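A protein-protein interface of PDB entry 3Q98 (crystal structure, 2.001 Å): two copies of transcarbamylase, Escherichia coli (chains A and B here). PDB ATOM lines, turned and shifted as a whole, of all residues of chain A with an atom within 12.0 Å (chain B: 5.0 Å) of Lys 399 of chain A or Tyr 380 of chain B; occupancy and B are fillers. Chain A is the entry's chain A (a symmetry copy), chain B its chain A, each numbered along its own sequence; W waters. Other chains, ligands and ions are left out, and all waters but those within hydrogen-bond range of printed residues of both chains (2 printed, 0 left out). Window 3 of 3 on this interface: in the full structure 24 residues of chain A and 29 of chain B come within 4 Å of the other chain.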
ATOM      1  N   ARG A  52      13.274  -7.512  29.832  1.00  0.00           N
ATOM      2  CA  ARG A  52      12.087  -7.776  30.624  1.00  0.00           C
ATOM      3  C   ARG A  52      11.679  -6.524  31.390  1.00  0.00           C
ATOM      4  O   ARG A  52      10.494  -6.204  31.478  1.00  0.00           O
ATOM      5  CB  ARG A  52      12.385  -8.941  31.565  1.00  0.00           C
ATOM      6  CG  ARG A  52      11.301  -9.318  32.570  1.00  0.00           C
ATOM      7  CD  ARG A  52      10.052  -9.801  31.907  1.00  0.00           C
ATOM      8  NE  ARG A  52       9.197 -10.568  32.813  1.00  0.00           N
ATOM      9  CZ  ARG A  52       8.618 -10.076  33.906  1.00  0.00           C
ATOM     10  NH1 ARG A  52       8.824  -8.815  34.261  1.00  0.00           N
ATOM     11  NH2 ARG A  52       7.838 -10.850  34.647  1.00  0.00           N
ATOM     12  N   GLU A  54      12.000  -3.435  30.595  1.00  0.00           N
ATOM     13  CA  GLU A  54      11.367  -2.419  29.760  1.00  0.00           C
ATOM     14  C   GLU A  54      10.210  -2.987  28.927  1.00  0.00           C
ATOM     15  O   GLU A  54       9.886  -2.463  27.856  1.00  0.00           O
ATOM     16  CB  GLU A  54      12.402  -1.728  28.868  1.00  0.00           C
ATOM     17  CG  GLU A  54      13.388  -0.841  29.633  1.00  0.00           C
ATOM     18  CD  GLU A  54      12.696   0.238  30.450  1.00  0.00           C
ATOM     19  OE1 GLU A  54      13.069   0.424  31.628  1.00  0.00           O
ATOM     20  OE2 GLU A  54      11.772   0.893  29.921  1.00  0.00           O
ATOM     21  N   ASN A  55       9.611  -4.067  29.416  1.00  0.00           N
ATOM     22  CA  ASN A  55       8.401  -4.626  28.807  1.00  0.00           C
ATOM     23  C   ASN A  55       8.606  -5.175  27.394  1.00  0.00           C
ATOM     24  O   ASN A  55       7.693  -5.140  26.573  1.00  0.00           O
ATOM     25  CB  ASN A  55       7.283  -3.576  28.785  1.00  0.00           C
ATOM     26  CG  ASN A  55       5.926  -4.190  28.541  1.00  0.00           C
ATOM     27  OD1 ASN A  55       5.699  -5.344  28.898  1.00  0.00           O
ATOM     28  ND2 ASN A  55       5.008  -3.420  27.942  1.00  0.00           N
ATOM     29  N   ILE A  56       9.806  -5.665  27.105  1.00  0.00           N
ATOM     30  CA  ILE A  56      10.058  -6.315  25.822  1.00  0.00           C
ATOM     31  C   ILE A  56      10.029  -7.833  25.993  1.00  0.00           C
ATOM     32  O   ILE A  56      10.717  -8.386  26.839  1.00  0.00           O
ATOM     33  CB  ILE A  56      11.396  -5.874  25.192  1.00  0.00           C
ATOM     34  CG1 ILE A  56      11.301  -4.420  24.721  1.00  0.00           C
ATOM     35  CG2 ILE A  56      11.770  -6.807  24.030  1.00  0.00           C
ATOM     36  CD1 ILE A  56      12.556  -3.887  24.047  1.00  0.00           C
ATOM     37  N   SER A  57       9.214  -8.494  25.185  1.00  0.00           N
ATOM     38  CA  SER A  57       9.049  -9.933  25.259  1.00  0.00           C
ATOM     39  C   SER A  57      10.330 -10.658  24.883  1.00  0.00           C
ATOM     40  O   SER A  57      10.978 -10.321  23.892  1.00  0.00           O
ATOM     41  CB  SER A  57       7.945 -10.363  24.287  1.00  0.00           C
ATOM     42  OG  SER A  57       7.875 -11.774  24.185  1.00  0.00           O
ATOM     43  N   LYS A  59      10.135 -14.034  24.485  1.00  0.00           N
ATOM     44  CA  LYS A  59       9.542 -15.316  24.136  1.00  0.00           C
ATOM     45  C   LYS A  59      10.264 -15.841  22.898  1.00  0.00           C
ATOM     46  O   LYS A  59      10.273 -15.204  21.852  1.00  0.00           O
ATOM     47  CB  LYS A  59       8.044 -15.124  23.892  1.00  0.00           C
ATOM     48  CG  LYS A  59       7.208 -16.382  23.670  1.00  0.00           C
ATOM     49  CD  LYS A  59       5.718 -16.007  23.715  1.00  0.00           C
ATOM     50  CE  LYS A  59       4.828 -17.105  23.152  1.00  0.00           C
ATOM     51  NZ  LYS A  59       4.789 -18.304  24.040  1.00  0.00           N
ATOM     52  N   ALA A 394      10.967  -5.938  19.419  1.00  0.00           N
ATOM     53  CA  ALA A 394      10.435  -5.195  20.556  1.00  0.00           C
ATOM     54  C   ALA A 394       8.946  -5.455  20.792  1.00  0.00           C
ATOM     55  O   ALA A 394       8.167  -4.524  21.020  1.00  0.00           O
ATOM     56  CB  ALA A 394      10.698  -3.700  20.389  1.00  0.00           C
ATOM     57  N   GLN A 395       8.559  -6.726  20.723  1.00  0.00           N
ATOM     58  CA  GLN A 395       7.209  -7.134  21.076  1.00  0.00           C
ATOM     59  C   GLN A 395       6.953  -6.859  22.563  1.00  0.00           C
ATOM     60  O   GLN A 395       7.787  -7.160  23.419  1.00  0.00           O
ATOM     61  CB  GLN A 395       7.004  -8.616  20.752  1.00  0.00           C
ATOM     62  CG  GLN A 395       5.755  -9.220  21.342  1.00  0.00           C
ATOM     63  CD  GLN A 395       4.493  -8.554  20.825  1.00  0.00           C
ATOM     64  OE1 GLN A 395       4.425  -8.145  19.661  1.00  0.00           O
ATOM     65  NE2 GLN A 395       3.484  -8.441  21.686  1.00  0.00           N
ATOM     66  N   GLU A 396       5.797  -6.289  22.881  1.00  0.00           N
ATOM     67  CA  GLU A 396       5.502  -5.979  24.279  1.00  0.00           C
ATOM     68  C   GLU A 396       5.226  -7.261  25.053  1.00  0.00           C
ATOM     69  O   GLU A 396       4.705  -8.226  24.491  1.00  0.00           O
ATOM     70  CB  GLU A 396       4.326  -5.001  24.390  1.00  0.00           C
ATOM     71  CG  GLU A 396       3.083  -5.420  23.635  1.00  0.00           C
ATOM     72  CD  GLU A 396       2.316  -4.232  23.086  1.00  0.00           C
ATOM     73  OE1 GLU A 396       2.883  -3.117  23.063  1.00  0.00           O
ATOM     74  OE2 GLU A 396       1.153  -4.412  22.671  1.00  0.00           O
ATOM     75  N   ARG A 397       5.601  -7.291  26.331  1.00  0.00           N
ATOM     76  CA  ARG A 397       5.214  -8.412  27.176  1.00  0.00           C
ATOM     77  C   ARG A 397       3.781  -8.229  27.644  1.00  0.00           C
ATOM     78  O   ARG A 397       2.974  -9.153  27.561  1.00  0.00           O
ATOM     79  CB  ARG A 397       6.131  -8.574  28.387  1.00  0.00           C
ATOM     80  CG  ARG A 397       5.758  -9.794  29.226  1.00  0.00           C
ATOM     81  CD  ARG A 397       6.544  -9.877  30.522  1.00  0.00           C
ATOM     82  NE  ARG A 397       5.742  -9.458  31.678  1.00  0.00           N
ATOM     83  CZ  ARG A 397       6.017  -8.402  32.428  1.00  0.00           C
ATOM     84  NH1 ARG A 397       7.074  -7.649  32.140  1.00  0.00           N
ATOM     85  NH2 ARG A 397       5.247  -8.096  33.468  1.00  0.00           N
ATOM     86  N   VAL A 398       3.467  -7.038  28.141  1.00  0.00           N
ATOM     87  CA  VAL A 398       2.097  -6.751  28.568  1.00  0.00           C
ATOM     88  C   VAL A 398       1.494  -5.660  27.690  1.00  0.00           C
ATOM     89  O   VAL A 398       2.145  -4.658  27.376  1.00  0.00           O
ATOM     90  CB  VAL A 398       1.994  -6.411  30.098  1.00  0.00           C
ATOM     91  CG1 VAL A 398       3.301  -6.729  30.810  1.00  0.00           C
ATOM     92  CG2 VAL A 398       1.596  -4.982  30.331  1.00  0.00           C
ATOM     93  N   LYS A 399       0.257  -5.884  27.269  1.00  0.00           N
ATOM     94  CA  LYS A 399      -0.401  -5.027  26.300  1.00  0.00           C
ATOM     95  C   LYS A 399      -0.713  -3.654  26.897  1.00  0.00           C
ATOM     96  O   LYS A 399      -0.869  -3.494  28.108  1.00  0.00           O
ATOM     97  CB  LYS A 399      -1.671  -5.713  25.786  1.00  0.00           C
ATOM     98  CG  LYS A 399      -2.141  -5.248  24.420  1.00  0.00           C
ATOM     99  CD  LYS A 399      -2.865  -6.377  23.685  1.00  0.00           C
ATOM    100  CE  LYS A 399      -1.947  -7.581  23.515  1.00  0.00           C
ATOM    101  NZ  LYS A 399      -2.591  -8.690  22.756  1.00  0.00           N
ATOM    102  OXT LYS A 399      -0.798  -2.659  26.179  1.00  0.00           O
ATOM    103  N   HIS B  23      -6.673   0.662  40.878  1.00  0.00           N
ATOM    104  CA  HIS B  23      -5.309   0.492  40.405  1.00  0.00           C
ATOM    105  C   HIS B  23      -4.279   0.847  41.483  1.00  0.00           C
ATOM    106  O   HIS B  23      -3.086   0.621  41.308  1.00  0.00           O
ATOM    107  CB  HIS B  23      -5.066   1.266  39.103  1.00  0.00           C
ATOM    108  CG  HIS B  23      -5.214   2.745  39.246  1.00  0.00           C
ATOM    109  ND1 HIS B  23      -6.439   3.355  39.414  1.00  0.00           N
ATOM    110  CD2 HIS B  23      -4.291   3.737  39.272  1.00  0.00           C
ATOM    111  CE1 HIS B  23      -6.265   4.660  39.532  1.00  0.00           C
ATOM    112  NE2 HIS B  23      -4.972   4.918  39.450  1.00  0.00           N
ATOM    113  N   LYS B  59      -5.963 -12.005  25.527  1.00  0.00           N
ATOM    114  CA  LYS B  59      -4.610 -12.220  26.015  1.00  0.00           C
ATOM    115  C   LYS B  59      -3.946 -10.854  26.165  1.00  0.00           C
ATOM    116  O   LYS B  59      -3.818 -10.103  25.205  1.00  0.00           O
ATOM    117  CB  LYS B  59      -3.860 -13.121  25.031  1.00  0.00           C
ATOM    118  CG  LYS B  59      -2.470 -13.597  25.445  1.00  0.00           C
ATOM    119  CD  LYS B  59      -2.004 -14.689  24.468  1.00  0.00           C
ATOM    120  CE  LYS B  59      -0.512 -14.964  24.575  1.00  0.00           C
ATOM    121  NZ  LYS B  59      -0.159 -15.640  25.858  1.00  0.00           N
ATOM    122  N   VAL B  60      -3.548 -10.532  27.385  1.00  0.00           N
ATOM    123  CA  VAL B  60      -2.921  -9.262  27.683  1.00  0.00           C
ATOM    124  C   VAL B  60      -1.426  -9.427  28.001  1.00  0.00           C
ATOM    125  O   VAL B  60      -0.641  -8.495  27.820  1.00  0.00           O
ATOM    126  CB  VAL B  60      -3.666  -8.574  28.832  1.00  0.00           C
ATOM    127  CG1 VAL B  60      -2.861  -7.447  29.411  1.00  0.00           C
ATOM    128  CG2 VAL B  60      -5.025  -8.086  28.341  1.00  0.00           C
ATOM    129  N   LEU B 376      -7.053  -7.199  35.915  1.00  0.00           N
ATOM    130  CA  LEU B 376      -6.986  -6.070  35.003  1.00  0.00           C
ATOM    131  C   LEU B 376      -7.234  -4.726  35.707  1.00  0.00           C
ATOM    132  O   LEU B 376      -6.631  -3.713  35.360  1.00  0.00           O
ATOM    133  CB  LEU B 376      -7.952  -6.258  33.835  1.00  0.00           C
ATOM    134  CG  LEU B 376      -7.646  -7.391  32.829  1.00  0.00           C
ATOM    135  CD1 LEU B 376      -8.711  -7.445  31.755  1.00  0.00           C
ATOM    136  CD2 LEU B 376      -6.294  -7.213  32.188  1.00  0.00           C
ATOM    137  N   SER B 377      -8.121  -4.722  36.694  1.00  0.00           N
ATOM    138  CA  SER B 377      -8.491  -3.492  37.382  1.00  0.00           C
ATOM    139  C   SER B 377      -7.378  -2.964  38.279  1.00  0.00           C
ATOM    140  O   SER B 377      -7.326  -1.765  38.583  1.00  0.00           O
ATOM    141  CB  SER B 377      -9.779  -3.694  38.184  1.00  0.00           C
ATOM    142  OG  SER B 377     -10.896  -3.717  37.322  1.00  0.00           O
ATOM    143  N   ARG B 378      -6.502  -3.862  38.716  1.00  0.00           N
ATOM    144  CA  ARG B 378      -5.313  -3.453  39.439  1.00  0.00           C
ATOM    145  C   ARG B 378      -4.237  -2.975  38.468  1.00  0.00           C
ATOM    146  O   ARG B 378      -3.548  -1.992  38.739  1.00  0.00           O
ATOM    147  CB  ARG B 378      -4.768  -4.586  40.304  1.00  0.00           C
ATOM    148  CG  ARG B 378      -3.237  -4.588  40.454  1.00  0.00           C
ATOM    149  CD  ARG B 378      -2.659  -3.318  41.105  1.00  0.00           C
ATOM    150  NE  ARG B 378      -2.868  -3.250  42.545  1.00  0.00           N
ATOM    151  CZ  ARG B 378      -2.197  -2.443  43.363  1.00  0.00           C
ATOM    152  NH1 ARG B 378      -1.253  -1.639  42.892  1.00  0.00           N
ATOM    153  NH2 ARG B 378      -2.459  -2.448  44.658  1.00  0.00           N
ATOM    154  N   LYS B 379      -4.101  -3.661  37.336  1.00  0.00           N
ATOM    155  CA  LYS B 379      -2.997  -3.377  36.407  1.00  0.00           C
ATOM    156  C   LYS B 379      -3.198  -2.139  35.516  1.00  0.00           C
ATOM    157  O   LYS B 379      -2.228  -1.476  35.111  1.00  0.00           O
ATOM    158  CB  LYS B 379      -2.705  -4.604  35.551  1.00  0.00           C
ATOM    159  CG  LYS B 379      -2.191  -5.778  36.359  1.00  0.00           C
ATOM    160  CD  LYS B 379      -0.838  -6.228  35.833  1.00  0.00           C
ATOM    161  CE  LYS B 379      -0.107  -7.098  36.841  1.00  0.00           C
ATOM    162  NZ  LYS B 379       0.426  -6.276  37.950  1.00  0.00           N
ATOM    163  N   TYR B 380      -4.449  -1.834  35.201  1.00  0.00           N
ATOM    164  CA  TYR B 380      -4.750  -0.673  34.377  1.00  0.00           C
ATOM    165  C   TYR B 380      -5.710   0.287  35.068  1.00  0.00           C
ATOM    166  O   TYR B 380      -6.806  -0.097  35.463  1.00  0.00           O
ATOM    167  CB  TYR B 380      -5.339  -1.106  33.042  1.00  0.00           C
ATOM    168  CG  TYR B 380      -4.439  -2.028  32.258  1.00  0.00           C
ATOM    169  CD1 TYR B 380      -3.559  -1.527  31.303  1.00  0.00           C
ATOM    170  CD2 TYR B 380      -4.465  -3.399  32.471  1.00  0.00           C
ATOM    171  CE1 TYR B 380      -2.741  -2.367  30.579  1.00  0.00           C
ATOM    172  CE2 TYR B 380      -3.640  -4.244  31.753  1.00  0.00           C
ATOM    173  CZ  TYR B 380      -2.783  -3.725  30.810  1.00  0.00           C
ATOM    174  OH  TYR B 380      -1.968  -4.571  30.093  1.00  0.00           O
ATOM    175  N   ALA B 381      -5.288   1.537  35.204  1.00  0.00           N
ATOM    176  CA  ALA B 381      -6.148   2.575  35.733  1.00  0.00           C
ATOM    177  C   ALA B 381      -7.420   2.692  34.899  1.00  0.00           C
ATOM    178  O   ALA B 381      -8.494   2.947  35.428  1.00  0.00           O
ATOM    179  CB  ALA B 381      -5.402   3.912  35.773  1.00  0.00           C
ATOM    180  N   LYS B 382      -7.291   2.493  33.593  1.00  0.00           N
ATOM    181  CA  LYS B 382      -8.431   2.600  32.686  1.00  0.00           C
ATOM    182  C   LYS B 382      -8.592   1.298  31.893  1.00  0.00           C
ATOM    183  O   LYS B 382      -8.147   1.196  30.758  1.00  0.00           O
ATOM    184  CB  LYS B 382      -8.266   3.801  31.744  1.00  0.00           C
ATOM    185  CG  LYS B 382      -8.853   5.120  32.252  1.00  0.00           C
ATOM    186  CD  LYS B 382      -8.428   5.417  33.678  1.00  0.00           C
ATOM    187  CE  LYS B 382      -8.790   6.835  34.097  1.00  0.00           C
ATOM    188  NZ  LYS B 382     -10.261   7.066  34.190  1.00  0.00           N
ATOM    189  N   PRO B 383      -9.228   0.286  32.503  1.00  0.00           N
ATOM    190  CA  PRO B 383      -9.395  -0.998  31.823  1.00  0.00           C
ATOM    191  C   PRO B 383     -10.219  -0.862  30.551  1.00  0.00           C
ATOM    192  O   PRO B 383     -10.172  -1.742  29.700  1.00  0.00           O
ATOM    193  CB  PRO B 383     -10.155  -1.846  32.853  1.00  0.00           C
ATOM    194  CG  PRO B 383      -9.936  -1.194  34.139  1.00  0.00           C
ATOM    195  CD  PRO B 383      -9.803   0.269  33.858  1.00  0.00           C
ATOM    196  N   LEU B 386      -7.949  -0.688  27.544  1.00  0.00           N
ATOM    197  CA  LEU B 386      -7.435  -2.011  27.209  1.00  0.00           C
ATOM    198  C   LEU B 386      -8.450  -2.877  26.462  1.00  0.00           C
ATOM    199  O   LEU B 386      -8.107  -3.515  25.475  1.00  0.00           O
ATOM    200  CB  LEU B 386      -6.951  -2.733  28.455  1.00  0.00           C
ATOM    201  CG  LEU B 386      -6.596  -4.193  28.209  1.00  0.00           C
ATOM    202  CD1 LEU B 386      -5.479  -4.312  27.181  1.00  0.00           C
ATOM    203  CD2 LEU B 386      -6.218  -4.861  29.515  1.00  0.00           C
ATOM    204  N   GLN B 389      -8.834  -1.747  22.855  1.00  0.00           N
ATOM    205  CA  GLN B 389      -7.701  -2.265  22.096  1.00  0.00           C
ATOM    206  C   GLN B 389      -7.891  -3.742  21.715  1.00  0.00           C
ATOM    207  O   GLN B 389      -7.699  -4.124  20.557  1.00  0.00           O
ATOM    208  CB  GLN B 389      -6.401  -2.082  22.882  1.00  0.00           C
ATOM    209  CG  GLN B 389      -5.161  -2.508  22.112  1.00  0.00           C
ATOM    210  CD  GLN B 389      -3.866  -2.275  22.880  1.00  0.00           C
ATOM    211  OE1 GLN B 389      -3.837  -1.533  23.862  1.00  0.00           O
ATOM    212  NE2 GLN B 389      -2.783  -2.905  22.421  1.00  0.00           N
ATOM    213  N   LEU B 390      -8.258  -4.567  22.691  1.00  0.00           N
ATOM    214  CA  LEU B 390      -8.547  -5.981  22.440  1.00  0.00           C
ATOM    215  C   LEU B 390      -9.639  -6.150  21.378  1.00  0.00           C
ATOM    216  O   LEU B 390      -9.526  -6.984  20.484  1.00  0.00           O
ATOM    217  CB  LEU B 390      -8.951  -6.687  23.739  1.00  0.00           C
ATOM    218  CG  LEU B 390      -7.836  -6.932  24.758  1.00  0.00           C
ATOM    219  CD1 LEU B 390      -8.405  -7.452  26.079  1.00  0.00           C
ATOM    220  CD2 LEU B 390      -6.815  -7.908  24.183  1.00  0.00           C
ATOM    221  N   GLU B 393      -8.249  -5.080  17.734  1.00  0.00           N
ATOM    222  CA  GLU B 393      -7.341  -6.093  17.204  1.00  0.00           C
ATOM    223  C   GLU B 393      -8.107  -7.348  16.802  1.00  0.00           C
ATOM    224  O   GLU B 393      -7.771  -8.000  15.818  1.00  0.00           O
ATOM    225  CB  GLU B 393      -6.257  -6.426  18.226  1.00  0.00           C
ATOM    226  CG  GLU B 393      -5.317  -5.256  18.474  1.00  0.00           C
ATOM    227  CD  GLU B 393      -4.362  -5.482  19.633  1.00  0.00           C
ATOM    228  OE1 GLU B 393      -4.365  -6.584  20.221  1.00  0.00           O
ATOM    229  OE2 GLU B 393      -3.603  -4.545  19.955  1.00  0.00           O
HETATM  230  O   HOH W   1      -5.421  -8.822  20.778  1.00  0.00           O
HETATM  231  O   HOH W   2       2.426 -16.238  25.294  1.00  0.00           O
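The backbone carbonyl oxygen of Lys 59 of chain B lies within hydrogen-bond range of the side-chain amino group of Lys 399 of chain A (3.1 Å). The backbone NH (N) of Lys 399 of chain A lies within hydrogen-bond range of the backbone carbonyl oxygen (O) of Val 60 of chain B. The side-chain hydroxyl of Tyr 380 of chain B lies within hydrogen-bond range of the chain-end carboxylate of Lys 399 of chain A, at 2.5 Å. OE1 of Glu 393 of chain B lies within salt-bridge range of NZ of Lys 399 of chain A (3.7 Å).
NE2 of Gln 389 of chain B lies within hydrogen-bond range of OE2 of Glu 393 of chain B (3.1 Å). The backbone carbonyl oxygen (O) of Asn 55 of chain A lies within hydrogen-bond range of the backbone NH (N) of Arg 397 of chain A (3.0 Å). The side-chain amide oxygen of Asn 55 of chain A lies within hydrogen-bond range of the backbone NH of Val 398 of chain A.
Among the printed residues, merely in contact across the chains: Lys 399 of chain A with Gln 389 of chain B (3.1 Å), Val 398 of chain A with Val 60 of chain B (3.3 Å), Val 398 of chain A with Tyr 380 of chain B (3.6 Å) and Arg 397 of chain A with Val 60 of chain B (3.7 Å).
Of the printed residues of chain B, Arg 397 of chain A touches Val 60. Printed residues of chain B within 4 Å of Val 398 of chain A: Val 60 (3.3 Å) and Tyr 380 (3.6 Å). Of chain B, only Lys 59, Val 60, Tyr 380, Gln 389 and Glu 393 come within 4 Å of Lys 399 of chain A. No residue of chain A comes within 4 Å of His 23 of chain B. Of the printed residues of chain A, Lys 59 of chain B touches Lys 399. No residue of chain A comes within 4 Å of Leu 376 of chain B. No residue of chain A comes within 4 Å of Ser 377 of chain B. No residue of chain A comes within 4 Å of Lys 379 of chain B. No residue of chain A comes within 4 Å of Ala 381 of chain B. No residue of chain A comes within 4 Å of Leu 386 of chain B. Of chain A, only Lys 399 (3.1 Å) comes within 4 Å of Gln 389 of chain B. Of the printed residues of chain A, Glu 393 of chain B touches Lys 399 (3.7 Å). The nearest printed residue of chain B that does not touch Lys 399 of chain A is Leu 390 of chain B (4.3 Å). The nearest residue of chain A that does not touch Tyr 380 of chain B is Arg 397 of chain A (7.2 Å). The nearest printed residue of chain B that does not touch Val 398 of chain A is Lys 379 of chain B (6.1 Å).
Printed residues of chain B that touch a printed residue of chain A: Lys 59, Val 60, Tyr 380, Gln 389 and Glu 393. Hydrophobic or aromatic side chains of chain B within 4 Å of the printed part of chain A: Tyr 380. Along chain A the printed residues that touch a printed residue of chain B span positions 397 to 399. Among the printed residues, Asp or Glu carboxylates within 4 Å of a Lys or Arg side-chain nitrogen of the other chain: Lys 399 of chain A with Glu 393 of chain B (3.7 Å).
Position printed for both chains: 59.
Water W1 lies within hydrogen-bond range of the side-chain carboxylate (OE1) of Glu 393 of chain B (2.5 Å) and the side-chain amino group (NZ) of Lys 399 of chain A (3.5 Å). Water W2 bridges the side-chain amino group of Lys 59 of chain B and the side-chain amino group of Lys 59 of chain A.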
